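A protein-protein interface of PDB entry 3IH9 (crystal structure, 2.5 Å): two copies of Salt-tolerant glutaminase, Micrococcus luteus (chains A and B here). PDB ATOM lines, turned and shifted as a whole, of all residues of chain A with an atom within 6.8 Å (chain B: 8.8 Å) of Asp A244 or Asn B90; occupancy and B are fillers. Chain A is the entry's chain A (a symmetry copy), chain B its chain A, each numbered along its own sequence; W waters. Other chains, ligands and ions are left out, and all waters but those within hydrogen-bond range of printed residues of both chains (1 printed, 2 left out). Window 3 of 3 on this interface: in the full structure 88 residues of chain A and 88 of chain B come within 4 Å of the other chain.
Of the 24 printed residues of chain B, 3 touch a printed residue of chain A.
Printed residues of chain B that touch a printed residue of chain A: Leu B89, Asn B90 and Pro B91.
Of the 13 printed residues of chain A, 3 touch a printed residue of chain B.
Water W1 lies within hydrogen-bond range of OG of Ser B239, O of Leu B89 and O of Gly A247.
7 positions are printed for both chains.
Of the 4 pairs that touch across the chains among the printed residues, none has its exchanged pair printed and touching as well.
Asn B90 touches just one residue of chain A: Asp A244 (3.8 Å).
No residue of chain B comes within 4 Å of Ala A245.
Of the printed residues of chain A, Leu B89 touches Gly A247 (3.6 Å) and Gln A248 (3.6 Å).
Printed residues of chain A within 4 Å of Pro B91: Gly A247.
Of the printed residues of chain B, Gly A247 touches Leu B89 (3.6 Å) and Pro B91 (3.99 Å).
Ser A92 touches none of the printed residues of chain B.
The nearest residue of chain B that does not touch Asp A244 is Pro B91 (5.2 Å).
The nearest printed residue of chain A that does not touch Pro B91 is Asp A244 (5.2 Å).
Among the printed residues, pairs that only touch across the chains: Gln A248 with Leu B89 (3.6 Å), Gly A247 with Leu B89 (3.6 Å), Asp A244 with Asn B90 (3.8 Å) and Gly A247 with Pro B91 (3.99 Å).
N of Leu B89 sits at hydrogen-bond distance from O of Asp B109, at 3.0 Å.
The backbone carbonyl oxygen (O) of Asp B109 is in hydrogen-bond range of the backbone NH (N) of Asn B90, 2.7 Å away.
The backbone carbonyl oxygen of Asn B90 lies close to the side-chain amide oxygen of Asn B110 (2.8 Å).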
ATOM      1  N   PRO A  91     -37.354  15.584 -17.746  1.00  0.00           N
ATOM      2  CA  PRO A  91     -37.841  15.662 -16.368  1.00  0.00           C
ATOM      3  C   PRO A  91     -38.248  17.081 -15.985  1.00  0.00           C
ATOM      4  O   PRO A  91     -37.655  18.052 -16.444  1.00  0.00           O
ATOM      5  CB  PRO A  91     -36.662  15.127 -15.547  1.00  0.00           C
ATOM      6  CG  PRO A  91     -35.472  15.358 -16.420  1.00  0.00           C
ATOM      7  CD  PRO A  91     -35.986  15.040 -17.795  1.00  0.00           C
ATOM      8  N   SER A  92     -39.286  17.196 -15.165  1.00  0.00           N
ATOM      9  CA  SER A  92     -39.753  18.500 -14.728  1.00  0.00           C
ATOM     10  C   SER A  92     -40.676  18.360 -13.522  1.00  0.00           C
ATOM     11  O   SER A  92     -41.104  17.246 -13.198  1.00  0.00           O
ATOM     12  CB  SER A  92     -40.493  19.193 -15.872  1.00  0.00           C
ATOM     13  OG  SER A  92     -41.889  19.226 -15.640  1.00  0.00           O
ATOM     14  N   GLY A  93     -40.959  19.484 -12.857  1.00  0.00           N
ATOM     15  CA  GLY A  93     -41.862  19.478 -11.711  1.00  0.00           C
ATOM     16  C   GLY A  93     -43.304  19.585 -12.208  1.00  0.00           C
ATOM     17  O   GLY A  93     -43.523  19.994 -13.346  1.00  0.00           O
ATOM     18  N   GLU A  94     -44.288  19.230 -11.385  1.00  0.00           N
ATOM     19  CA  GLU A  94     -45.688  19.303 -11.818  1.00  0.00           C
ATOM     20  C   GLU A  94     -46.146  20.738 -12.102  1.00  0.00           C
ATOM     21  O   GLU A  94     -47.109  20.954 -12.835  1.00  0.00           O
ATOM     22  CB  GLU A  94     -46.607  18.644 -10.781  1.00  0.00           C
ATOM     23  CG  GLU A  94     -48.120  18.655 -11.119  1.00  0.00           C
ATOM     24  CD  GLU A  94     -48.481  17.986 -12.464  1.00  0.00           C
ATOM     25  OE1 GLU A  94     -48.230  16.773 -12.641  1.00  0.00           O
ATOM     26  OE2 GLU A  94     -49.030  18.680 -13.348  1.00  0.00           O
ATOM     27  N   SER A 239     -36.399   8.722 -14.589  1.00  0.00           N
ATOM     28  CA  SER A 239     -35.973  10.104 -14.769  1.00  0.00           C
ATOM     29  C   SER A 239     -37.010  11.147 -14.424  1.00  0.00           C
ATOM     30  O   SER A 239     -36.662  12.291 -14.131  1.00  0.00           O
ATOM     31  CB  SER A 239     -35.511  10.331 -16.209  1.00  0.00           C
ATOM     32  OG  SER A 239     -36.615  10.401 -17.085  1.00  0.00           O
ATOM     33  N   SER A 240     -38.283  10.761 -14.434  1.00  0.00           N
ATOM     34  CA  SER A 240     -39.344  11.727 -14.165  1.00  0.00           C
ATOM     35  C   SER A 240     -40.332  11.372 -13.071  1.00  0.00           C
ATOM     36  O   SER A 240     -41.058  12.234 -12.590  1.00  0.00           O
ATOM     37  CB  SER A 240     -40.112  11.998 -15.466  1.00  0.00           C
ATOM     38  OG  SER A 240     -39.232  12.362 -16.518  1.00  0.00           O
ATOM     39  N   MET A 242     -40.167  11.049  -9.939  1.00  0.00           N
ATOM     40  CA  MET A 242     -40.115  11.866  -8.729  1.00  0.00           C
ATOM     41  C   MET A 242     -39.832  13.333  -9.035  1.00  0.00           C
ATOM     42  O   MET A 242     -39.309  14.077  -8.201  1.00  0.00           O
ATOM     43  CB  MET A 242     -39.072  11.302  -7.761  1.00  0.00           C
ATOM     44  CG  MET A 242     -39.364   9.869  -7.304  1.00  0.00           C
ATOM     45  SD  MET A 242     -40.831   9.766  -6.256  1.00  0.00           S
ATOM     46  CE  MET A 242     -41.309   8.017  -6.427  1.00  0.00           C
ATOM     47  N   TYR A 243     -40.216  13.729 -10.247  1.00  0.00           N
ATOM     48  CA  TYR A 243     -40.078  15.091 -10.747  1.00  0.00           C
ATOM     49  C   TYR A 243     -38.705  15.720 -10.545  1.00  0.00           C
ATOM     50  O   TYR A 243     -37.708  15.182 -11.016  1.00  0.00           O
ATOM     51  CB  TYR A 243     -41.160  15.978 -10.125  1.00  0.00           C
ATOM     52  CG  TYR A 243     -42.533  15.347 -10.134  1.00  0.00           C
ATOM     53  CD1 TYR A 243     -42.930  14.493  -9.111  1.00  0.00           C
ATOM     54  CD2 TYR A 243     -43.423  15.573 -11.185  1.00  0.00           C
ATOM     55  CE1 TYR A 243     -44.181  13.878  -9.128  1.00  0.00           C
ATOM     56  CE2 TYR A 243     -44.680  14.956 -11.216  1.00  0.00           C
ATOM     57  CZ  TYR A 243     -45.050  14.111 -10.180  1.00  0.00           C
ATOM     58  OH  TYR A 243     -46.284  13.499 -10.194  1.00  0.00           O
ATOM     59  N   ASP A 244     -38.650  16.864  -9.865  1.00  0.00           N
ATOM     60  CA  ASP A 244     -37.369  17.536  -9.636  1.00  0.00           C
ATOM     61  C   ASP A 244     -36.480  16.851  -8.592  1.00  0.00           C
ATOM     62  O   ASP A 244     -35.312  17.209  -8.445  1.00  0.00           O
ATOM     63  CB  ASP A 244     -37.575  19.009  -9.237  1.00  0.00           C
ATOM     64  CG  ASP A 244     -37.974  19.897 -10.412  1.00  0.00           C
ATOM     65  OD1 ASP A 244     -37.437  19.725 -11.533  1.00  0.00           O
ATOM     66  OD2 ASP A 244     -38.822  20.792 -10.204  1.00  0.00           O
ATOM     67  N   ALA A 245     -37.019  15.875  -7.867  1.00  0.00           N
ATOM     68  CA  ALA A 245     -36.227  15.158  -6.868  1.00  0.00           C
ATOM     69  C   ALA A 245     -35.738  13.820  -7.424  1.00  0.00           C
ATOM     70  O   ALA A 245     -35.131  13.023  -6.706  1.00  0.00           O
ATOM     71  CB  ALA A 245     -37.047  14.929  -5.599  1.00  0.00           C
ATOM     72  N   ALA A 246     -35.989  13.592  -8.713  1.00  0.00           N
ATOM     73  CA  ALA A 246     -35.598  12.352  -9.398  1.00  0.00           C
ATOM     74  C   ALA A 246     -34.119  11.974  -9.271  1.00  0.00           C
ATOM     75  O   ALA A 246     -33.784  10.791  -9.154  1.00  0.00           O
ATOM     76  CB  ALA A 246     -35.991  12.432 -10.884  1.00  0.00           C
ATOM     77  N   GLY A 247     -33.239  12.970  -9.317  1.00  0.00           N
ATOM     78  CA  GLY A 247     -31.816  12.698  -9.184  1.00  0.00           C
ATOM     79  C   GLY A 247     -31.495  12.175  -7.789  1.00  0.00           C
ATOM     80  O   GLY A 247     -30.897  11.114  -7.640  1.00  0.00           O
ATOM     81  N   GLN A 248     -31.898  12.924  -6.767  1.00  0.00           N
ATOM     82  CA  GLN A 248     -31.672  12.525  -5.380  1.00  0.00           C
ATOM     83  C   GLN A 248     -32.267  11.136  -5.147  1.00  0.00           C
ATOM     84  O   GLN A 248     -31.646  10.267  -4.531  1.00  0.00           O
ATOM     85  CB  GLN A 248     -32.335  13.525  -4.435  1.00  0.00           C
ATOM     86  CG  GLN A 248     -32.198  13.177  -2.969  1.00  0.00           C
ATOM     87  CD  GLN A 248     -31.298  14.151  -2.207  1.00  0.00           C
ATOM     88  OE1 GLN A 248     -30.993  13.935  -1.032  1.00  0.00           O
ATOM     89  NE2 GLN A 248     -30.879  15.226  -2.869  1.00  0.00           N
ATOM     90  N   TYR B  71     -14.748  12.326  -7.641  1.00  0.00           N
ATOM     91  CA  TYR B  71     -15.936  12.279  -6.795  1.00  0.00           C
ATOM     92  C   TYR B  71     -15.811  11.012  -5.973  1.00  0.00           C
ATOM     93  O   TYR B  71     -16.047  10.998  -4.763  1.00  0.00           O
ATOM     94  CB  TYR B  71     -17.188  12.214  -7.675  1.00  0.00           C
ATOM     95  CG  TYR B  71     -18.522  12.223  -6.950  1.00  0.00           C
ATOM     96  CD1 TYR B  71     -18.707  12.963  -5.781  1.00  0.00           C
ATOM     97  CD2 TYR B  71     -19.624  11.581  -7.499  1.00  0.00           C
ATOM     98  CE1 TYR B  71     -19.961  13.073  -5.185  1.00  0.00           C
ATOM     99  CE2 TYR B  71     -20.887  11.682  -6.916  1.00  0.00           C
ATOM    100  CZ  TYR B  71     -21.050  12.433  -5.761  1.00  0.00           C
ATOM    101  OH  TYR B  71     -22.306  12.578  -5.216  1.00  0.00           O
ATOM    102  N   VAL B  87     -21.589  18.938  -2.008  1.00  0.00           N
ATOM    103  CA  VAL B  87     -22.055  18.608  -3.346  1.00  0.00           C
ATOM    104  C   VAL B  87     -23.441  17.978  -3.352  1.00  0.00           C
ATOM    105  O   VAL B  87     -23.693  17.007  -2.655  1.00  0.00           O
ATOM    106  CB  VAL B  87     -21.081  17.648  -4.043  1.00  0.00           C
ATOM    107  CG1 VAL B  87     -21.390  17.583  -5.534  1.00  0.00           C
ATOM    108  CG2 VAL B  87     -19.661  18.104  -3.808  1.00  0.00           C
ATOM    109  N   GLY B  88     -24.333  18.528  -4.165  1.00  0.00           N
ATOM    110  CA  GLY B  88     -25.683  17.996  -4.245  1.00  0.00           C
ATOM    111  C   GLY B  88     -25.817  16.820  -5.195  1.00  0.00           C
ATOM    112  O   GLY B  88     -24.822  16.294  -5.708  1.00  0.00           O
ATOM    113  N   LEU B  89     -27.062  16.411  -5.430  1.00  0.00           N
ATOM    114  CA  LEU B  89     -27.369  15.288  -6.304  1.00  0.00           C
ATOM    115  C   LEU B  89     -28.427  15.702  -7.328  1.00  0.00           C
ATOM    116  O   LEU B  89     -29.100  14.858  -7.925  1.00  0.00           O
ATOM    117  CB  LEU B  89     -27.884  14.119  -5.467  1.00  0.00           C
ATOM    118  CG  LEU B  89     -26.960  13.658  -4.327  1.00  0.00           C
ATOM    119  CD1 LEU B  89     -27.734  12.834  -3.331  1.00  0.00           C
ATOM    120  CD2 LEU B  89     -25.814  12.863  -4.883  1.00  0.00           C
ATOM    121  N   ASN B  90     -28.564  17.005  -7.541  1.00  0.00           N
ATOM    122  CA  ASN B  90     -29.549  17.500  -8.484  1.00  0.00           C
ATOM    123  C   ASN B  90     -29.048  17.773  -9.890  1.00  0.00           C
ATOM    124  O   ASN B  90     -28.055  18.465 -10.091  1.00  0.00           O
ATOM    125  CB  ASN B  90     -30.214  18.759  -7.934  1.00  0.00           C
ATOM    126  CG  ASN B  90     -31.104  18.459  -6.749  1.00  0.00           C
ATOM    127  OD1 ASN B  90     -31.891  17.505  -6.772  1.00  0.00           O
ATOM    128  ND2 ASN B  90     -30.995  19.274  -5.706  1.00  0.00           N
ATOM    129  N   PRO B  91     -29.733  17.215 -10.891  1.00  0.00           N
ATOM    130  CA  PRO B  91     -29.309  17.444 -12.272  1.00  0.00           C
ATOM    131  C   PRO B  91     -29.485  18.901 -12.691  1.00  0.00           C
ATOM    132  O   PRO B  91     -30.412  19.574 -12.252  1.00  0.00           O
ATOM    133  CB  PRO B  91     -30.181  16.473 -13.075  1.00  0.00           C
ATOM    134  CG  PRO B  91     -31.371  16.242 -12.202  1.00  0.00           C
ATOM    135  CD  PRO B  91     -30.781  16.182 -10.822  1.00  0.00           C
ATOM    136  N   SER B  92     -28.570  19.391 -13.517  1.00  0.00           N
ATOM    137  CA  SER B  92     -28.647  20.763 -13.987  1.00  0.00           C
ATOM    138  C   SER B  92     -27.736  20.966 -15.194  1.00  0.00           C
ATOM    139  O   SER B  92     -26.906  20.100 -15.494  1.00  0.00           O
ATOM    140  CB  SER B  92     -28.241  21.716 -12.863  1.00  0.00           C
ATOM    141  OG  SER B  92     -26.966  22.286 -13.103  1.00  0.00           O
ATOM    142  N   GLY B  93     -27.910  22.096 -15.887  1.00  0.00           N
ATOM    143  CA  GLY B  93     -27.071  22.415 -17.036  1.00  0.00           C
ATOM    144  C   GLY B  93     -25.787  23.088 -16.549  1.00  0.00           C
ATOM    145  O   GLY B  93     -25.750  23.577 -15.422  1.00  0.00           O
ATOM    146  N   SER B 100     -28.655  28.556  -7.085  1.00  0.00           N
ATOM    147  CA  SER B 100     -28.342  27.190  -6.712  1.00  0.00           C
ATOM    148  C   SER B 100     -27.555  27.087  -5.379  1.00  0.00           C
ATOM    149  O   SER B 100     -27.620  26.018  -4.787  1.00  0.00           O
ATOM    150  CB  SER B 100     -27.653  26.443  -7.872  1.00  0.00           C
ATOM    151  OG  SER B 100     -26.325  26.883  -8.126  1.00  0.00           O
ATOM    152  N   ALA B 103     -29.855  28.388  -1.815  1.00  0.00           N
ATOM    153  CA  ALA B 103     -30.748  27.401  -1.208  1.00  0.00           C
ATOM    154  C   ALA B 103     -30.183  27.080   0.177  1.00  0.00           C
ATOM    155  O   ALA B 103     -28.981  27.268   0.400  1.00  0.00           O
ATOM    156  CB  ALA B 103     -30.788  26.148  -2.094  1.00  0.00           C
ATOM    157  N   SER B 105     -29.027  24.718   1.296  1.00  0.00           N
ATOM    158  CA  SER B 105     -28.003  23.697   1.118  1.00  0.00           C
ATOM    159  C   SER B 105     -26.716  24.438   1.024  1.00  0.00           C
ATOM    160  O   SER B 105     -25.720  24.123   1.651  1.00  0.00           O
ATOM    161  CB  SER B 105     -28.229  22.982  -0.205  1.00  0.00           C
ATOM    162  OG  SER B 105     -29.545  22.497  -0.276  1.00  0.00           O
ATOM    163  N   ARG B 107     -24.968  24.701  -1.799  1.00  0.00           N
ATOM    164  CA  ARG B 107     -24.035  23.805  -2.484  1.00  0.00           C
ATOM    165  C   ARG B 107     -24.337  23.611  -3.974  1.00  0.00           C
ATOM    166  O   ARG B 107     -25.478  23.706  -4.410  1.00  0.00           O
ATOM    167  CB  ARG B 107     -24.020  22.442  -1.793  1.00  0.00           C
ATOM    168  CG  ARG B 107     -25.348  21.724  -1.887  1.00  0.00           C
ATOM    169  CD  ARG B 107     -25.397  20.497  -1.014  1.00  0.00           C
ATOM    170  NE  ARG B 107     -26.707  19.868  -1.097  1.00  0.00           N
ATOM    171  CZ  ARG B 107     -27.141  18.921  -0.274  1.00  0.00           C
ATOM    172  NH1 ARG B 107     -26.365  18.487   0.713  1.00  0.00           N
ATOM    173  NH2 ARG B 107     -28.350  18.400  -0.448  1.00  0.00           N
ATOM    174  N   PRO B 108     -23.298  23.361  -4.778  1.00  0.00           N
ATOM    175  CA  PRO B 108     -23.524  23.159  -6.213  1.00  0.00           C
ATOM    176  C   PRO B 108     -24.412  21.925  -6.438  1.00  0.00           C
ATOM    177  O   PRO B 108     -24.375  20.977  -5.642  1.00  0.00           O
ATOM    178  CB  PRO B 108     -22.102  23.017  -6.770  1.00  0.00           C
ATOM    179  CG  PRO B 108     -21.290  22.556  -5.577  1.00  0.00           C
ATOM    180  CD  PRO B 108     -21.858  23.379  -4.461  1.00  0.00           C
ATOM    181  N   ASP B 109     -25.204  21.958  -7.514  1.00  0.00           N
ATOM    182  CA  ASP B 109     -26.159  20.898  -7.855  1.00  0.00           C
ATOM    183  C   ASP B 109     -25.664  19.454  -7.874  1.00  0.00           C
ATOM    184  O   ASP B 109     -26.350  18.560  -7.368  1.00  0.00           O
ATOM    185  CB  ASP B 109     -26.842  21.204  -9.202  1.00  0.00           C
ATOM    186  CG  ASP B 109     -27.935  22.259  -9.085  1.00  0.00           C
ATOM    187  OD1 ASP B 109     -28.644  22.278  -8.054  1.00  0.00           O
ATOM    188  OD2 ASP B 109     -28.105  23.062 -10.029  1.00  0.00           O
ATOM    189  N   ASN B 110     -24.498  19.211  -8.463  1.00  0.00           N
ATOM    190  CA  ASN B 110     -23.964  17.856  -8.501  1.00  0.00           C
ATOM    191  C   ASN B 110     -22.501  17.828  -8.934  1.00  0.00           C
ATOM    192  O   ASN B 110     -21.945  18.830  -9.372  1.00  0.00           O
ATOM    193  CB  ASN B 110     -24.798  16.979  -9.441  1.00  0.00           C
ATOM    194  CG  ASN B 110     -24.787  17.484 -10.861  1.00  0.00           C
ATOM    195  OD1 ASN B 110     -25.546  18.370 -11.219  1.00  0.00           O
ATOM    196  ND2 ASN B 110     -23.906  16.933 -11.674  1.00  0.00           N
ATOM    197  N   ALA B 111     -21.891  16.658  -8.832  1.00  0.00           N
ATOM    198  CA  ALA B 111     -20.487  16.482  -9.165  1.00  0.00           C
ATOM    199  C   ALA B 111     -20.123  16.447 -10.652  1.00  0.00           C
ATOM    200  O   ALA B 111     -18.945  16.410 -10.986  1.00  0.00           O
ATOM    201  CB  ALA B 111     -19.963  15.221  -8.473  1.00  0.00           C
ATOM    202  N   MET B 112     -21.103  16.466 -11.548  1.00  0.00           N
ATOM    203  CA  MET B 112     -20.769  16.412 -12.967  1.00  0.00           C
ATOM    204  C   MET B 112     -20.520  17.786 -13.577  1.00  0.00           C
ATOM    205  O   MET B 112     -19.838  17.904 -14.595  1.00  0.00           O
ATOM    206  CB  MET B 112     -21.866  15.678 -13.765  1.00  0.00           C
ATOM    207  CG  MET B 112     -22.133  14.224 -13.337  1.00  0.00           C
ATOM    208  SD  MET B 112     -20.658  13.190 -12.994  1.00  0.00           S
ATOM    209  CE  MET B 112     -19.725  13.436 -14.433  1.00  0.00           C
ATOM    210  N   ILE B 113     -21.073  18.832 -12.971  1.00  0.00           N
ATOM    211  CA  ILE B 113     -20.862  20.185 -13.486  1.00  0.00           C
ATOM    212  C   ILE B 113     -19.612  20.801 -12.854  1.00  0.00           C
ATOM    213  O   ILE B 113     -19.227  20.444 -11.741  1.00  0.00           O
ATOM    214  CB  ILE B 113     -22.060  21.088 -13.203  1.00  0.00           C
ATOM    215  CG1 ILE B 113     -22.315  21.161 -11.692  1.00  0.00           C
ATOM    216  CG2 ILE B 113     -23.269  20.555 -13.934  1.00  0.00           C
ATOM    217  CD1 ILE B 113     -23.261  22.256 -11.285  1.00  0.00           C
ATOM    218  N   VAL B 236     -25.056   9.336 -10.233  1.00  0.00           N
ATOM    219  CA  VAL B 236     -24.924  10.718 -10.667  1.00  0.00           C
ATOM    220  C   VAL B 236     -24.516  10.855 -12.126  1.00  0.00           C
ATOM    221  O   VAL B 236     -24.842  11.850 -12.772  1.00  0.00           O
ATOM    222  CB  VAL B 236     -23.923  11.482  -9.771  1.00  0.00           C
ATOM    223  CG1 VAL B 236     -23.645  12.877 -10.346  1.00  0.00           C
ATOM    224  CG2 VAL B 236     -24.488  11.588  -8.357  1.00  0.00           C
ATOM    225  N   SER B 239     -27.922  10.452 -13.882  1.00  0.00           N
ATOM    226  CA  SER B 239     -28.854  11.561 -13.731  1.00  0.00           C
ATOM    227  C   SER B 239     -28.304  12.918 -14.106  1.00  0.00           C
ATOM    228  O   SER B 239     -29.069  13.829 -14.424  1.00  0.00           O
ATOM    229  CB  SER B 239     -29.375  11.624 -12.295  1.00  0.00           C
ATOM    230  OG  SER B 239     -28.389  12.140 -11.427  1.00  0.00           O
ATOM    231  N   SER B 240     -26.982  13.060 -14.093  1.00  0.00           N
ATOM    232  CA  SER B 240     -26.379  14.356 -14.389  1.00  0.00           C
ATOM    233  C   SER B 240     -25.327  14.389 -15.479  1.00  0.00           C
ATOM    234  O   SER B 240     -24.992  15.454 -15.984  1.00  0.00           O
ATOM    235  CB  SER B 240     -25.785  14.935 -13.099  1.00  0.00           C
ATOM    236  OG  SER B 240     -26.741  14.952 -12.051  1.00  0.00           O
ATOM    237  N   GLY B 241     -24.797  13.233 -15.846  1.00  0.00           N
ATOM    238  CA  GLY B 241     -23.779  13.193 -16.877  1.00  0.00           C
ATOM    239  C   GLY B 241     -24.085  13.965 -18.148  1.00  0.00           C
ATOM    240  O   GLY B 241     -23.187  14.563 -18.719  1.00  0.00           O
ATOM    241  N   TYR B 243     -26.339  16.447 -18.358  1.00  0.00           N
ATOM    242  CA  TYR B 243     -26.999  17.659 -17.889  1.00  0.00           C
ATOM    243  C   TYR B 243     -28.508  17.698 -18.099  1.00  0.00           C
ATOM    244  O   TYR B 243     -29.218  16.825 -17.611  1.00  0.00           O
ATOM    245  CB  TYR B 243     -26.346  18.883 -18.536  1.00  0.00           C
ATOM    246  CG  TYR B 243     -24.835  18.838 -18.520  1.00  0.00           C
ATOM    247  CD1 TYR B 243     -24.132  18.182 -19.524  1.00  0.00           C
ATOM    248  CD2 TYR B 243     -24.109  19.417 -17.479  1.00  0.00           C
ATOM    249  CE1 TYR B 243     -22.740  18.104 -19.499  1.00  0.00           C
ATOM    250  CE2 TYR B 243     -22.711  19.340 -17.439  1.00  0.00           C
ATOM    251  CZ  TYR B 243     -22.036  18.682 -18.456  1.00  0.00           C
ATOM    252  OH  TYR B 243     -20.661  18.600 -18.434  1.00  0.00           O
ATOM    253  N   ASP B 244     -29.001  18.714 -18.806  1.00  0.00           N
ATOM    254  CA  ASP B 244     -30.442  18.828 -19.044  1.00  0.00           C
ATOM    255  C   ASP B 244     -30.988  17.826 -20.068  1.00  0.00           C
ATOM    256  O   ASP B 244     -32.202  17.697 -20.217  1.00  0.00           O
ATOM    257  CB  ASP B 244     -30.824  20.254 -19.478  1.00  0.00           C
ATOM    258  CG  ASP B 244     -30.809  21.255 -18.326  1.00  0.00           C
ATOM    259  OD1 ASP B 244     -31.242  20.913 -17.199  1.00  0.00           O
ATOM    260  OD2 ASP B 244     -30.376  22.404 -18.560  1.00  0.00           O
HETATM  261  O   HOH W   1     -27.972  12.359  -8.887  1.00  0.00           O
